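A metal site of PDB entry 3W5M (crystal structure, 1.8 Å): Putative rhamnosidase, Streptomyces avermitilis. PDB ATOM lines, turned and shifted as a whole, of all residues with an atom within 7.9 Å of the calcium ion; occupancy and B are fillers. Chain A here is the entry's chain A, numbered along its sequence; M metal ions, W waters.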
ATOM      1  N   TRP A 142      -4.115 -28.900 -22.967  1.00  0.00           N
ATOM      2  CA  TRP A 142      -3.804 -29.198 -21.584  1.00  0.00           C
ATOM      3  C   TRP A 142      -2.687 -30.216 -21.559  1.00  0.00           C
ATOM      4  O   TRP A 142      -2.209 -30.631 -22.601  1.00  0.00           O
ATOM      5  CB  TRP A 142      -5.074 -29.740 -20.868  1.00  0.00           C
ATOM      6  CG  TRP A 142      -4.998 -29.701 -19.402  1.00  0.00           C
ATOM      7  CD1 TRP A 142      -4.975 -30.785 -18.557  1.00  0.00           C
ATOM      8  CD2 TRP A 142      -4.958 -28.537 -18.563  1.00  0.00           C
ATOM      9  NE1 TRP A 142      -4.920 -30.363 -17.252  1.00  0.00           N
ATOM     10  CE2 TRP A 142      -4.900 -29.000 -17.220  1.00  0.00           C
ATOM     11  CE3 TRP A 142      -4.946 -27.161 -18.812  1.00  0.00           C
ATOM     12  CZ2 TRP A 142      -4.825 -28.119 -16.121  1.00  0.00           C
ATOM     13  CZ3 TRP A 142      -4.884 -26.275 -17.709  1.00  0.00           C
ATOM     14  CH2 TRP A 142      -4.823 -26.778 -16.382  1.00  0.00           C
ATOM     15  N   PRO A 148      -9.383 -33.797 -20.984  1.00  0.00           N
ATOM     16  CA  PRO A 148      -9.457 -32.572 -20.186  1.00  0.00           C
ATOM     17  C   PRO A 148     -10.687 -31.690 -20.429  1.00  0.00           C
ATOM     18  O   PRO A 148     -11.124 -30.987 -19.506  1.00  0.00           O
ATOM     19  CB  PRO A 148      -8.147 -31.840 -20.546  1.00  0.00           C
ATOM     20  CG  PRO A 148      -7.257 -32.913 -21.097  1.00  0.00           C
ATOM     21  CD  PRO A 148      -8.171 -33.834 -21.828  1.00  0.00           C
ATOM     22  N   ALA A 152     -10.479 -32.760 -15.663  1.00  0.00           N
ATOM     23  CA  ALA A 152      -9.067 -32.797 -15.337  1.00  0.00           C
ATOM     24  C   ALA A 152      -8.955 -32.516 -13.838  1.00  0.00           C
ATOM     25  O   ALA A 152      -9.878 -31.936 -13.262  1.00  0.00           O
ATOM     26  CB  ALA A 152      -8.316 -31.738 -16.153  1.00  0.00           C
ATOM     27  N   PRO A 153      -7.829 -32.946 -13.199  1.00  0.00           N
ATOM     28  CA  PRO A 153      -7.662 -32.659 -11.762  1.00  0.00           C
ATOM     29  C   PRO A 153      -7.577 -31.159 -11.486  1.00  0.00           C
ATOM     30  O   PRO A 153      -7.273 -30.372 -12.399  1.00  0.00           O
ATOM     31  CB  PRO A 153      -6.310 -33.324 -11.427  1.00  0.00           C
ATOM     32  CG  PRO A 153      -5.596 -33.492 -12.751  1.00  0.00           C
ATOM     33  CD  PRO A 153      -6.709 -33.755 -13.736  1.00  0.00           C
ATOM     34  N   ALA A 154      -7.830 -30.757 -10.232  1.00  0.00           N
ATOM     35  CA  ALA A 154      -7.630 -29.373  -9.812  1.00  0.00           C
ATOM     36  C   ALA A 154      -6.134 -29.161  -9.539  1.00  0.00           C
ATOM     37  O   ALA A 154      -5.656 -29.295  -8.397  1.00  0.00           O
ATOM     38  CB  ALA A 154      -8.436 -29.073  -8.549  1.00  0.00           C
ATOM     39  N   ALA A 178      -7.947 -18.996 -20.406  1.00  0.00           N
ATOM     40  CA  ALA A 178      -7.784 -20.326 -19.796  1.00  0.00           C
ATOM     41  C   ALA A 178      -8.947 -20.646 -18.890  1.00  0.00           C
ATOM     42  O   ALA A 178      -9.487 -19.758 -18.243  1.00  0.00           O
ATOM     43  CB  ALA A 178      -6.477 -20.421 -19.003  1.00  0.00           C
ATOM     44  N   ASP A 179      -9.300 -21.922 -18.884  1.00  0.00           N
ATOM     45  CA  ASP A 179     -10.133 -22.504 -17.847  1.00  0.00           C
ATOM     46  C   ASP A 179      -9.163 -23.228 -16.886  1.00  0.00           C
ATOM     47  O   ASP A 179      -8.748 -24.347 -17.193  1.00  0.00           O
ATOM     48  CB  ASP A 179     -11.064 -23.521 -18.532  1.00  0.00           C
ATOM     49  CG  ASP A 179     -12.066 -24.159 -17.561  1.00  0.00           C
ATOM     50  OD1 ASP A 179     -11.814 -24.116 -16.355  1.00  0.00           O
ATOM     51  OD2 ASP A 179     -13.064 -24.734 -18.008  1.00  0.00           O
ATOM     52  N   ASN A 180      -8.775 -22.646 -15.742  1.00  0.00           N
ATOM     53  CA  ASN A 180      -9.336 -21.413 -15.177  1.00  0.00           C
ATOM     54  C   ASN A 180      -8.451 -20.193 -15.181  1.00  0.00           C
ATOM     55  O   ASN A 180      -8.957 -19.064 -15.320  1.00  0.00           O
ATOM     56  CB  ASN A 180      -9.785 -21.662 -13.728  1.00  0.00           C
ATOM     57  CG  ASN A 180     -10.945 -22.618 -13.676  1.00  0.00           C
ATOM     58  OD1 ASN A 180     -10.769 -23.826 -13.445  1.00  0.00           O
ATOM     59  ND2 ASN A 180     -12.147 -22.116 -13.976  1.00  0.00           N
ATOM     60  N   VAL A 181      -7.140 -20.380 -15.017  1.00  0.00           N
ATOM     61  CA  VAL A 181      -6.223 -19.227 -14.983  1.00  0.00           C
ATOM     62  C   VAL A 181      -4.903 -19.533 -15.686  1.00  0.00           C
ATOM     63  O   VAL A 181      -4.565 -20.704 -15.914  1.00  0.00           O
ATOM     64  CB  VAL A 181      -5.896 -18.759 -13.544  1.00  0.00           C
ATOM     65  CG1 VAL A 181      -7.131 -18.201 -12.843  1.00  0.00           C
ATOM     66  CG2 VAL A 181      -5.241 -19.866 -12.723  1.00  0.00           C
ATOM     67  N   ASP A 199     -10.826 -15.212 -10.209  1.00  0.00           N
ATOM     68  CA  ASP A 199     -11.515 -15.850 -11.332  1.00  0.00           C
ATOM     69  C   ASP A 199     -13.007 -16.061 -11.092  1.00  0.00           C
ATOM     70  O   ASP A 199     -13.417 -16.660 -10.098  1.00  0.00           O
ATOM     71  CB  ASP A 199     -10.862 -17.196 -11.729  1.00  0.00           C
ATOM     72  CG  ASP A 199     -11.647 -17.921 -12.847  1.00  0.00           C
ATOM     73  OD1 ASP A 199     -11.992 -17.280 -13.854  1.00  0.00           O
ATOM     74  OD2 ASP A 199     -11.916 -19.142 -12.713  1.00  0.00           O
ATOM     75  N   TRP A 203     -12.494 -17.787 -18.383  1.00  0.00           N
ATOM     76  CA  TRP A 203     -12.264 -18.395 -19.702  1.00  0.00           C
ATOM     77  C   TRP A 203     -13.186 -17.819 -20.777  1.00  0.00           C
ATOM     78  O   TRP A 203     -12.865 -17.879 -21.977  1.00  0.00           O
ATOM     79  CB  TRP A 203     -12.400 -19.919 -19.642  1.00  0.00           C
ATOM     80  CG  TRP A 203     -13.723 -20.397 -19.137  1.00  0.00           C
ATOM     81  CD1 TRP A 203     -14.034 -20.765 -17.860  1.00  0.00           C
ATOM     82  CD2 TRP A 203     -14.912 -20.575 -19.910  1.00  0.00           C
ATOM     83  NE1 TRP A 203     -15.359 -21.160 -17.792  1.00  0.00           N
ATOM     84  CE2 TRP A 203     -15.918 -21.063 -19.048  1.00  0.00           C
ATOM     85  CE3 TRP A 203     -15.212 -20.386 -21.268  1.00  0.00           C
ATOM     86  CZ2 TRP A 203     -17.210 -21.364 -19.497  1.00  0.00           C
ATOM     87  CZ3 TRP A 203     -16.500 -20.682 -21.709  1.00  0.00           C
ATOM     88  CH2 TRP A 203     -17.475 -21.168 -20.826  1.00  0.00           C
ATOM     89  N   SER A 227      -3.843 -23.225 -14.427  1.00  0.00           N
ATOM     90  CA  SER A 227      -4.370 -23.969 -13.284  1.00  0.00           C
ATOM     91  C   SER A 227      -5.849 -24.238 -13.450  1.00  0.00           C
ATOM     92  O   SER A 227      -6.604 -23.376 -13.907  1.00  0.00           O
ATOM     93  CB  SER A 227      -4.105 -23.224 -11.977  1.00  0.00           C
ATOM     94  OG  SER A 227      -2.700 -23.050 -11.800  1.00  0.00           O
ATOM     95  N   ASN A 228      -6.257 -25.441 -13.064  1.00  0.00           N
ATOM     96  CA  ASN A 228      -7.686 -25.775 -13.057  1.00  0.00           C
ATOM     97  C   ASN A 228      -8.148 -25.654 -11.619  1.00  0.00           C
ATOM     98  O   ASN A 228      -7.502 -26.200 -10.712  1.00  0.00           O
ATOM     99  CB  ASN A 228      -7.861 -27.204 -13.567  1.00  0.00           C
ATOM    100  CG  ASN A 228      -9.328 -27.636 -13.686  1.00  0.00           C
ATOM    101  OD1 ASN A 228     -10.240 -26.818 -13.762  1.00  0.00           O
ATOM    102  ND2 ASN A 228      -9.545 -28.949 -13.732  1.00  0.00           N
ATOM    103  N   ALA A 229      -9.246 -24.933 -11.394  1.00  0.00           N
ATOM    104  CA  ALA A 229      -9.687 -24.540 -10.041  1.00  0.00           C
ATOM    105  C   ALA A 229     -10.378 -25.643  -9.257  1.00  0.00           C
ATOM    106  O   ALA A 229     -10.384 -25.646  -8.008  1.00  0.00           O
ATOM    107  CB  ALA A 229     -10.582 -23.319 -10.126  1.00  0.00           C
ATOM    108  N   SER A 230     -10.968 -26.588  -9.957  1.00  0.00           N
ATOM    109  CA  SER A 230     -11.631 -27.704  -9.326  1.00  0.00           C
ATOM    110  C   SER A 230     -11.711 -28.844 -10.331  1.00  0.00           C
ATOM    111  O   SER A 230     -11.496 -28.639 -11.526  1.00  0.00           O
ATOM    112  CB  SER A 230     -13.048 -27.295  -8.901  1.00  0.00           C
ATOM    113  OG  SER A 230     -13.774 -26.916 -10.036  1.00  0.00           O
ATOM    114  N   VAL A 231     -12.020 -30.043  -9.858  1.00  0.00           N
ATOM    115  CA  VAL A 231     -12.137 -31.187 -10.747  1.00  0.00           C
ATOM    116  C   VAL A 231     -13.266 -30.924 -11.751  1.00  0.00           C
ATOM    117  O   VAL A 231     -14.402 -30.626 -11.372  1.00  0.00           O
ATOM    118  CB  VAL A 231     -12.394 -32.494  -9.955  1.00  0.00           C
ATOM    119  CG1 VAL A 231     -12.667 -33.655 -10.890  1.00  0.00           C
ATOM    120  CG2 VAL A 231     -11.188 -32.819  -9.086  1.00  0.00           C
ATOM    121  N   GLY A 232     -12.922 -31.041 -13.033  1.00  0.00           N
ATOM    122  CA  GLY A 232     -13.794 -30.684 -14.124  1.00  0.00           C
ATOM    123  C   GLY A 232     -12.942 -30.183 -15.278  1.00  0.00           C
ATOM    124  O   GLY A 232     -11.720 -30.356 -15.246  1.00  0.00           O
ATOM    125  N   PRO A 233     -13.569 -29.570 -16.293  1.00  0.00           N
ATOM    126  CA  PRO A 233     -12.890 -29.164 -17.552  1.00  0.00           C
ATOM    127  C   PRO A 233     -11.704 -28.216 -17.349  1.00  0.00           C
ATOM    128  O   PRO A 233     -11.731 -27.358 -16.481  1.00  0.00           O
ATOM    129  CB  PRO A 233     -13.996 -28.484 -18.353  1.00  0.00           C
ATOM    130  CG  PRO A 233     -15.270 -29.072 -17.829  1.00  0.00           C
ATOM    131  CD  PRO A 233     -15.037 -29.348 -16.364  1.00  0.00           C
ATOM    132  N   ALA A 234     -10.655 -28.428 -18.132  1.00  0.00           N
ATOM    133  CA  ALA A 234      -9.497 -27.559 -18.099  1.00  0.00           C
ATOM    134  C   ALA A 234      -8.968 -27.450 -19.488  1.00  0.00           C
ATOM    135  O   ALA A 234      -9.110 -28.369 -20.312  1.00  0.00           O
ATOM    136  CB  ALA A 234      -8.405 -28.091 -17.175  1.00  0.00           C
ATOM    137  N   GLY A 235      -8.338 -26.313 -19.757  1.00  0.00           N
ATOM    138  CA  GLY A 235      -7.686 -26.102 -21.031  1.00  0.00           C
ATOM    139  C   GLY A 235      -7.309 -24.637 -21.161  1.00  0.00           C
ATOM    140  O   GLY A 235      -7.912 -23.774 -20.502  1.00  0.00           O
ATOM    141  N   TRP A 292     -16.678 -24.969 -24.070  1.00  0.00           N
ATOM    142  CA  TRP A 292     -16.374 -23.551 -23.983  1.00  0.00           C
ATOM    143  C   TRP A 292     -17.011 -22.684 -25.080  1.00  0.00           C
ATOM    144  O   TRP A 292     -17.124 -21.465 -24.903  1.00  0.00           O
ATOM    145  CB  TRP A 292     -14.863 -23.332 -23.934  1.00  0.00           C
ATOM    146  CG  TRP A 292     -14.191 -24.056 -22.806  1.00  0.00           C
ATOM    147  CD1 TRP A 292     -14.302 -23.772 -21.474  1.00  0.00           C
ATOM    148  CD2 TRP A 292     -13.294 -25.169 -22.911  1.00  0.00           C
ATOM    149  NE1 TRP A 292     -13.544 -24.662 -20.735  1.00  0.00           N
ATOM    150  CE2 TRP A 292     -12.893 -25.512 -21.590  1.00  0.00           C
ATOM    151  CE3 TRP A 292     -12.766 -25.898 -24.000  1.00  0.00           C
ATOM    152  CZ2 TRP A 292     -12.013 -26.555 -21.321  1.00  0.00           C
ATOM    153  CZ3 TRP A 292     -11.870 -26.941 -23.728  1.00  0.00           C
ATOM    154  CH2 TRP A 292     -11.505 -27.257 -22.403  1.00  0.00           C
HETATM  155 CA    CA M   1     -12.092 -25.726 -14.678  1.00  0.00          CA
HETATM  156  O   HOH W   1     -13.242 -27.397 -13.367  1.00  0.00           O
HETATM  157  O   HOH W   2     -14.032 -24.485 -13.499  1.00  0.00           O
HETATM  158  O   HOH W   3     -14.420 -25.619 -15.882  1.00  0.00           O
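The calcium ion is bound by the side-chain amide oxygen of Asn 228 (2.3 Å), the side-chain carboxylate of Asp 179 (2.3 Å), water W1 (2.4 Å), the backbone carbonyl oxygen of Pro 233 (2.5 Å), water W2 (2.6 Å), water W3 (2.6 Å) and the side-chain amide oxygen of Asn 180 (2.6 Å).
Along chain A the residues within 4 Å of the calcium ion span positions 179 to 233.
The side-chain amide nitrogen of Asn 228 sits at hydrogen-bond distance from the backbone carbonyl oxygen of Gly 232 (3.0 Å). ND2 of Asn 228 is in hydrogen-bond range of O of Ala 152. The side-chain amide nitrogen of Asn 228 lies within hydrogen-bond range of the backbone carbonyl oxygen of Pro 153, at 3.0 Å. The side-chain carboxylate (OD2) of Asp 179 sits at hydrogen-bond distance from the indole nitrogen (NE1) of Trp 292. The backbone NH (N) of Asp 179 lies within hydrogen-bond range of the backbone carbonyl oxygen (O) of Gly 235 (2.8 Å). OD1 of Asn 180 sits close to N of Ala 229 (2.8 Å). N of Asn 180 is in hydrogen-bond range of O of Ser 227, 2.9 Å away. ND2 of Asn 180 lies within hydrogen-bond range of OD2 of Asp 199 (3.2 Å).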
